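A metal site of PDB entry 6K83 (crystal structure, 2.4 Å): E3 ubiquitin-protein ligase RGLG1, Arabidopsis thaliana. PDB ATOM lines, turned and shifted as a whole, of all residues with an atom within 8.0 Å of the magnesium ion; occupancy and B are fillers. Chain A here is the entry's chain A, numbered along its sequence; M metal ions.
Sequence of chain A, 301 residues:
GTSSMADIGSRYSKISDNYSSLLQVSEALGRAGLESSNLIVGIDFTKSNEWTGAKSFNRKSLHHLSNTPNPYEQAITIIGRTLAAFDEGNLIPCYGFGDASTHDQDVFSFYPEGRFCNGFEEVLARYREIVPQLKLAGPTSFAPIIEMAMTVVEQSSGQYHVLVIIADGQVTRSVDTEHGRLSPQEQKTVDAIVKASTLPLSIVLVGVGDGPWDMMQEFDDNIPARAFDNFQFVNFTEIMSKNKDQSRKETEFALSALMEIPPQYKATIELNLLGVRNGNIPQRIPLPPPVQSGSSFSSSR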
ATOM      1  N   ASP A  44      -2.878 -10.925 -30.124  1.00  0.00           N
ATOM      2  CA  ASP A  44      -4.092 -10.132 -30.097  1.00  0.00           C
ATOM      3  C   ASP A  44      -4.138  -9.296 -28.840  1.00  0.00           C
ATOM      4  O   ASP A  44      -4.276  -9.829 -27.733  1.00  0.00           O
ATOM      5  CB  ASP A  44      -5.319 -11.051 -30.176  1.00  0.00           C
ATOM      6  CG  ASP A  44      -6.579 -10.389 -29.649  1.00  0.00           C
ATOM      7  OD1 ASP A  44      -6.922  -9.324 -30.162  1.00  0.00           O
ATOM      8  OD2 ASP A  44      -7.221 -10.910 -28.717  1.00  0.00           O
ATOM      9  N   PHE A  45      -4.000  -7.986 -28.995  1.00  0.00           N
ATOM     10  CA  PHE A  45      -4.068  -7.078 -27.871  1.00  0.00           C
ATOM     11  C   PHE A  45      -5.372  -6.265 -27.855  1.00  0.00           C
ATOM     12  O   PHE A  45      -5.361  -5.108 -27.476  1.00  0.00           O
ATOM     13  CB  PHE A  45      -2.869  -6.123 -27.889  1.00  0.00           C
ATOM     14  CG  PHE A  45      -1.537  -6.792 -27.643  1.00  0.00           C
ATOM     15  CD1 PHE A  45      -1.238  -7.340 -26.393  1.00  0.00           C
ATOM     16  CD2 PHE A  45      -0.575  -6.850 -28.648  1.00  0.00           C
ATOM     17  CE1 PHE A  45      -0.009  -7.933 -26.162  1.00  0.00           C
ATOM     18  CE2 PHE A  45       0.649  -7.436 -28.412  1.00  0.00           C
ATOM     19  CZ  PHE A  45       0.935  -7.980 -27.163  1.00  0.00           C
ATOM     20  N   THR A  46      -6.480  -6.888 -28.241  1.00  0.00           N
ATOM     21  CA  THR A  46      -7.741  -6.181 -28.221  1.00  0.00           C
ATOM     22  C   THR A  46      -8.410  -6.236 -26.861  1.00  0.00           C
ATOM     23  O   THR A  46      -8.204  -7.167 -26.102  1.00  0.00           O
ATOM     24  CB  THR A  46      -8.709  -6.730 -29.262  1.00  0.00           C
ATOM     25  OG1 THR A  46      -9.077  -8.089 -28.937  1.00  0.00           O
ATOM     26  CG2 THR A  46      -8.093  -6.660 -30.642  1.00  0.00           C
ATOM     27  N   LYS A  47      -9.256  -5.248 -26.581  1.00  0.00           N
ATOM     28  CA  LYS A  47      -9.899  -5.126 -25.274  1.00  0.00           C
ATOM     29  C   LYS A  47     -10.779  -6.322 -24.851  1.00  0.00           C
ATOM     30  O   LYS A  47     -11.158  -6.433 -23.680  1.00  0.00           O
ATOM     31  CB  LYS A  47     -10.735  -3.850 -25.241  1.00  0.00           C
ATOM     32  CG  LYS A  47     -11.193  -3.436 -23.850  1.00  0.00           C
ATOM     33  CD  LYS A  47     -11.952  -2.120 -23.916  1.00  0.00           C
ATOM     34  CE  LYS A  47     -12.435  -1.693 -22.551  1.00  0.00           C
ATOM     35  NZ  LYS A  47     -13.048  -0.337 -22.637  1.00  0.00           N
ATOM     36  N   SER A  48     -11.094  -7.237 -25.756  1.00  0.00           N
ATOM     37  CA  SER A  48     -11.949  -8.325 -25.341  1.00  0.00           C
ATOM     38  C   SER A  48     -11.206  -9.283 -24.410  1.00  0.00           C
ATOM     39  O   SER A  48     -11.845 -10.031 -23.682  1.00  0.00           O
ATOM     40  CB  SER A  48     -12.533  -9.081 -26.551  1.00  0.00           C
ATOM     41  OG  SER A  48     -11.564  -9.390 -27.531  1.00  0.00           O
ATOM     42  N   ASN A  49      -9.873  -9.221 -24.421  1.00  0.00           N
ATOM     43  CA  ASN A  49      -9.076 -10.019 -23.489  1.00  0.00           C
ATOM     44  C   ASN A  49      -9.358  -9.667 -22.018  1.00  0.00           C
ATOM     45  O   ASN A  49      -8.967 -10.397 -21.123  1.00  0.00           O
ATOM     46  CB  ASN A  49      -7.563  -9.869 -23.737  1.00  0.00           C
ATOM     47  CG  ASN A  49      -7.092 -10.498 -25.041  1.00  0.00           C
ATOM     48  OD1 ASN A  49      -7.121 -11.731 -25.230  1.00  0.00           O
ATOM     49  ND2 ASN A  49      -6.610  -9.642 -25.963  1.00  0.00           N
ATOM     50  N   GLU A  50     -10.030  -8.545 -21.765  1.00  0.00           N
ATOM     51  CA  GLU A  50     -10.335  -8.191 -20.383  1.00  0.00           C
ATOM     52  C   GLU A  50     -11.472  -9.046 -19.774  1.00  0.00           C
ATOM     53  O   GLU A  50     -11.503  -9.245 -18.550  1.00  0.00           O
ATOM     54  CB  GLU A  50     -10.676  -6.703 -20.284  1.00  0.00           C
ATOM     55  CG  GLU A  50      -9.433  -5.802 -20.458  1.00  0.00           C
ATOM     56  CD  GLU A  50      -9.751  -4.318 -20.387  1.00  0.00           C
ATOM     57  OE1 GLU A  50     -10.929  -3.946 -20.600  1.00  0.00           O
ATOM     58  OE2 GLU A  50      -8.828  -3.514 -20.102  1.00  0.00           O
ATOM     59  N   TRP A  51     -12.374  -9.584 -20.600  1.00  0.00           N
ATOM     60  CA  TRP A  51     -13.471 -10.390 -20.045  1.00  0.00           C
ATOM     61  C   TRP A  51     -13.477 -11.862 -20.458  1.00  0.00           C
ATOM     62  O   TRP A  51     -14.160 -12.681 -19.830  1.00  0.00           O
ATOM     63  CB  TRP A  51     -14.818  -9.771 -20.404  1.00  0.00           C
ATOM     64  CG  TRP A  51     -15.089  -9.622 -21.890  1.00  0.00           C
ATOM     65  CD1 TRP A  51     -15.532 -10.586 -22.761  1.00  0.00           C
ATOM     66  CD2 TRP A  51     -14.949  -8.418 -22.651  1.00  0.00           C
ATOM     67  NE1 TRP A  51     -15.669 -10.045 -24.033  1.00  0.00           N
ATOM     68  CE2 TRP A  51     -15.317  -8.717 -23.986  1.00  0.00           C
ATOM     69  CE3 TRP A  51     -14.536  -7.114 -22.351  1.00  0.00           C
ATOM     70  CZ2 TRP A  51     -15.288  -7.766 -25.011  1.00  0.00           C
ATOM     71  CZ3 TRP A  51     -14.510  -6.170 -23.370  1.00  0.00           C
ATOM     72  CH2 TRP A  51     -14.874  -6.503 -24.678  1.00  0.00           C
ATOM     73  N   THR A  52     -12.716 -12.231 -21.482  1.00  0.00           N
ATOM     74  CA  THR A  52     -12.756 -13.607 -21.955  1.00  0.00           C
ATOM     75  C   THR A  52     -11.936 -14.535 -21.071  1.00  0.00           C
ATOM     76  O   THR A  52     -11.752 -15.700 -21.413  1.00  0.00           O
ATOM     77  CB  THR A  52     -12.254 -13.707 -23.390  1.00  0.00           C
ATOM     78  OG1 THR A  52     -10.945 -13.138 -23.451  1.00  0.00           O
ATOM     79  CG2 THR A  52     -13.194 -12.943 -24.325  1.00  0.00           C
ATOM     80  N   TYR A  72      -1.361 -16.056 -22.499  1.00  0.00           N
ATOM     81  CA  TYR A  72      -0.460 -15.659 -23.568  1.00  0.00           C
ATOM     82  C   TYR A  72       0.978 -16.110 -23.277  1.00  0.00           C
ATOM     83  O   TYR A  72       1.634 -16.681 -24.151  1.00  0.00           O
ATOM     84  CB  TYR A  72      -0.545 -14.148 -23.833  1.00  0.00           C
ATOM     85  CG  TYR A  72      -1.795 -13.782 -24.628  1.00  0.00           C
ATOM     86  CD1 TYR A  72      -1.778 -13.790 -26.023  1.00  0.00           C
ATOM     87  CD2 TYR A  72      -3.000 -13.492 -23.990  1.00  0.00           C
ATOM     88  CE1 TYR A  72      -2.920 -13.494 -26.744  1.00  0.00           C
ATOM     89  CE2 TYR A  72      -4.153 -13.184 -24.719  1.00  0.00           C
ATOM     90  CZ  TYR A  72      -4.105 -13.183 -26.090  1.00  0.00           C
ATOM     91  OH  TYR A  72      -5.255 -12.890 -26.817  1.00  0.00           O
ATOM     92  N   PHE A  97      -1.510  -6.690 -32.695  1.00  0.00           N
ATOM     93  CA  PHE A  97      -2.624  -5.976 -33.296  1.00  0.00           C
ATOM     94  C   PHE A  97      -3.780  -5.777 -32.313  1.00  0.00           C
ATOM     95  O   PHE A  97      -4.009  -6.583 -31.422  1.00  0.00           O
ATOM     96  CB  PHE A  97      -3.116  -6.707 -34.550  1.00  0.00           C
ATOM     97  CG  PHE A  97      -3.562  -8.121 -34.322  1.00  0.00           C
ATOM     98  CD1 PHE A  97      -2.666  -9.176 -34.405  1.00  0.00           C
ATOM     99  CD2 PHE A  97      -4.902  -8.403 -34.047  1.00  0.00           C
ATOM    100  CE1 PHE A  97      -3.097 -10.494 -34.201  1.00  0.00           C
ATOM    101  CE2 PHE A  97      -5.341  -9.722 -33.831  1.00  0.00           C
ATOM    102  CZ  PHE A  97      -4.430 -10.751 -33.909  1.00  0.00           C
ATOM    103  N   GLY A  98      -4.499  -4.673 -32.501  1.00  0.00           N
ATOM    104  CA  GLY A  98      -5.741  -4.465 -31.783  1.00  0.00           C
ATOM    105  C   GLY A  98      -5.645  -3.603 -30.534  1.00  0.00           C
ATOM    106  O   GLY A  98      -6.598  -3.483 -29.770  1.00  0.00           O
ATOM    107  N   ALA A 137      -7.466  -2.264 -27.226  1.00  0.00           N
ATOM    108  CA  ALA A 137      -8.601  -1.686 -27.916  1.00  0.00           C
ATOM    109  C   ALA A 137      -9.324  -2.665 -28.853  1.00  0.00           C
ATOM    110  O   ALA A 137      -9.684  -3.783 -28.465  1.00  0.00           O
ATOM    111  CB  ALA A 137      -8.153  -0.449 -28.704  1.00  0.00           C
ATOM    112  N   GLY A 138      -9.528  -2.217 -30.087  1.00  0.00           N
ATOM    113  CA  GLY A 138     -10.278  -2.944 -31.090  1.00  0.00           C
ATOM    114  C   GLY A 138     -10.609  -1.987 -32.238  1.00  0.00           C
ATOM    115  O   GLY A 138     -10.038  -0.896 -32.334  1.00  0.00           O
ATOM    116  N   PRO A 139     -11.540  -2.405 -33.126  1.00  0.00           N
ATOM    117  CA  PRO A 139     -12.222  -3.711 -33.105  1.00  0.00           C
ATOM    118  C   PRO A 139     -11.286  -4.859 -33.457  1.00  0.00           C
ATOM    119  O   PRO A 139     -10.094  -4.667 -33.691  1.00  0.00           O
ATOM    120  CB  PRO A 139     -13.315  -3.562 -34.156  1.00  0.00           C
ATOM    121  CG  PRO A 139     -13.352  -2.084 -34.521  1.00  0.00           C
ATOM    122  CD  PRO A 139     -11.964  -1.586 -34.267  1.00  0.00           C
ATOM    123  N   THR A 140     -11.827  -6.070 -33.491  1.00  0.00           N
ATOM    124  CA  THR A 140     -10.995  -7.233 -33.649  1.00  0.00           C
ATOM    125  C   THR A 140     -11.098  -7.774 -35.049  1.00  0.00           C
ATOM    126  O   THR A 140     -12.173  -8.146 -35.493  1.00  0.00           O
ATOM    127  CB  THR A 140     -11.377  -8.337 -32.659  1.00  0.00           C
ATOM    128  OG1 THR A 140     -11.184  -7.853 -31.321  1.00  0.00           O
ATOM    129  CG2 THR A 140     -10.508  -9.585 -32.885  1.00  0.00           C
ATOM    130  N   SER A 141      -9.969  -7.830 -35.730  1.00  0.00           N
ATOM    131  CA  SER A 141      -9.912  -8.414 -37.052  1.00  0.00           C
ATOM    132  C   SER A 141      -8.583  -9.146 -37.218  1.00  0.00           C
ATOM    133  O   SER A 141      -7.565  -8.720 -36.670  1.00  0.00           O
ATOM    134  CB  SER A 141     -10.090  -7.317 -38.100  1.00  0.00           C
ATOM    135  OG  SER A 141      -9.836  -7.758 -39.415  1.00  0.00           O
ATOM    136  N   PHE A 142      -8.579 -10.249 -37.959  1.00  0.00           N
ATOM    137  CA  PHE A 142      -7.360 -10.973 -38.240  1.00  0.00           C
ATOM    138  C   PHE A 142      -6.741 -10.607 -39.572  1.00  0.00           C
ATOM    139  O   PHE A 142      -5.764 -11.202 -39.976  1.00  0.00           O
ATOM    140  CB  PHE A 142      -7.598 -12.471 -38.202  1.00  0.00           C
ATOM    141  CG  PHE A 142      -7.914 -13.002 -36.830  1.00  0.00           C
ATOM    142  CD1 PHE A 142      -7.628 -12.223 -35.713  1.00  0.00           C
ATOM    143  CD2 PHE A 142      -8.486 -14.254 -36.653  1.00  0.00           C
ATOM    144  CE1 PHE A 142      -7.917 -12.684 -34.455  1.00  0.00           C
ATOM    145  CE2 PHE A 142      -8.766 -14.734 -35.382  1.00  0.00           C
ATOM    146  CZ  PHE A 142      -8.491 -13.945 -34.289  1.00  0.00           C
ATOM    147  N   ALA A 167      -4.756 -15.542 -29.669  1.00  0.00           N
ATOM    148  CA  ALA A 167      -5.920 -14.680 -29.651  1.00  0.00           C
ATOM    149  C   ALA A 167      -7.074 -15.346 -28.906  1.00  0.00           C
ATOM    150  O   ALA A 167      -7.064 -16.565 -28.677  1.00  0.00           O
ATOM    151  CB  ALA A 167      -6.339 -14.320 -31.059  1.00  0.00           C
ATOM    152  N   ASP A 168      -8.080 -14.537 -28.566  1.00  0.00           N
ATOM    153  CA  ASP A 168      -9.230 -15.012 -27.818  1.00  0.00           C
ATOM    154  C   ASP A 168     -10.411 -15.383 -28.735  1.00  0.00           C
ATOM    155  O   ASP A 168     -11.511 -15.643 -28.256  1.00  0.00           O
ATOM    156  CB  ASP A 168      -9.648 -13.954 -26.769  1.00  0.00           C
ATOM    157  CG  ASP A 168     -10.462 -12.796 -27.363  1.00  0.00           C
ATOM    158  OD1 ASP A 168     -10.587 -12.659 -28.612  1.00  0.00           O
ATOM    159  OD2 ASP A 168     -10.976 -11.984 -26.549  1.00  0.00           O
ATOM    160  N   GLY A 169     -10.170 -15.368 -30.043  1.00  0.00           N
ATOM    161  CA  GLY A 169     -11.128 -15.852 -31.036  1.00  0.00           C
ATOM    162  C   GLY A 169     -12.355 -14.975 -31.265  1.00  0.00           C
ATOM    163  O   GLY A 169     -13.282 -15.349 -31.988  1.00  0.00           O
ATOM    164  N   GLN A 170     -12.367 -13.796 -30.646  1.00  0.00           N
ATOM    165  CA  GLN A 170     -13.564 -12.965 -30.725  1.00  0.00           C
ATOM    166  C   GLN A 170     -13.446 -11.904 -31.825  1.00  0.00           C
ATOM    167  O   GLN A 170     -13.198 -10.736 -31.543  1.00  0.00           O
ATOM    168  CB  GLN A 170     -13.829 -12.304 -29.364  1.00  0.00           C
ATOM    169  CG  GLN A 170     -13.865 -13.304 -28.208  1.00  0.00           C
ATOM    170  CD  GLN A 170     -14.742 -14.510 -28.532  1.00  0.00           C
ATOM    171  OE1 GLN A 170     -15.914 -14.363 -28.850  1.00  0.00           O
ATOM    172  NE2 GLN A 170     -14.160 -15.700 -28.470  1.00  0.00           N
ATOM    173  N   VAL A 171     -13.608 -12.316 -33.080  1.00  0.00           N
ATOM    174  CA  VAL A 171     -13.588 -11.358 -34.181  1.00  0.00           C
ATOM    175  C   VAL A 171     -14.902 -10.585 -34.185  1.00  0.00           C
ATOM    176  O   VAL A 171     -15.978 -11.172 -34.034  1.00  0.00           O
ATOM    177  CB  VAL A 171     -13.375 -12.027 -35.573  1.00  0.00           C
ATOM    178  CG1 VAL A 171     -13.426 -10.984 -36.665  1.00  0.00           C
ATOM    179  CG2 VAL A 171     -12.037 -12.755 -35.618  1.00  0.00           C
ATOM    180  N   THR A 172     -14.797  -9.281 -34.330  1.00  0.00           N
ATOM    181  CA  THR A 172     -15.926  -8.379 -34.186  1.00  0.00           C
ATOM    182  C   THR A 172     -17.051  -8.770 -35.152  1.00  0.00           C
ATOM    183  O   THR A 172     -16.837  -8.999 -36.344  1.00  0.00           O
ATOM    184  CB  THR A 172     -15.514  -6.929 -34.418  1.00  0.00           C
ATOM    185  OG1 THR A 172     -14.573  -6.548 -33.394  1.00  0.00           O
ATOM    186  CG2 THR A 172     -16.737  -6.003 -34.332  1.00  0.00           C
HETATM  187 MG    MG M   1     -11.160  -8.647 -29.240  1.00  0.00          MG
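Gln 170 touches the magnesium ion (O to MG, 3.7 Å).
Within 4 Å of the magnesium ion: Thr 46, Ser 48, Thr 140 and Gln 170.
Along chain A the residues within 4 Å of the magnesium ion span positions 46 to 170.
The magnesium ion is bound by the side-chain hydroxyl of Ser 48 (1.9 Å), the side-chain hydroxyl of Thr 46 (2.2 Å) and the side-chain hydroxyl of Thr 140 (2.2 Å).
The magnesium ion has three donor atoms within binding distance.
OD2 of Asp 168 sits close to OG of Ser 48, at 2.8 Å.
OG1 of Thr 52 sits at hydrogen-bond distance from O of Ser 48, at 3.2 Å.
The backbone NH of Thr 46 lies close to the side-chain carboxylate of Asp 44, 3.1 Å away.
The backbone carbonyl oxygen of Thr 46 is in hydrogen-bond range of the side-chain amide nitrogen of Asn 49 (2.9 Å).
The side-chain hydroxyl (OG1) of Thr 172 is in hydrogen-bond range of the backbone NH (N) of Thr 140, at 2.8 Å.
NE2 of Gln 170 lies within hydrogen-bond range of O of Asp 168 (2.7 Å).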
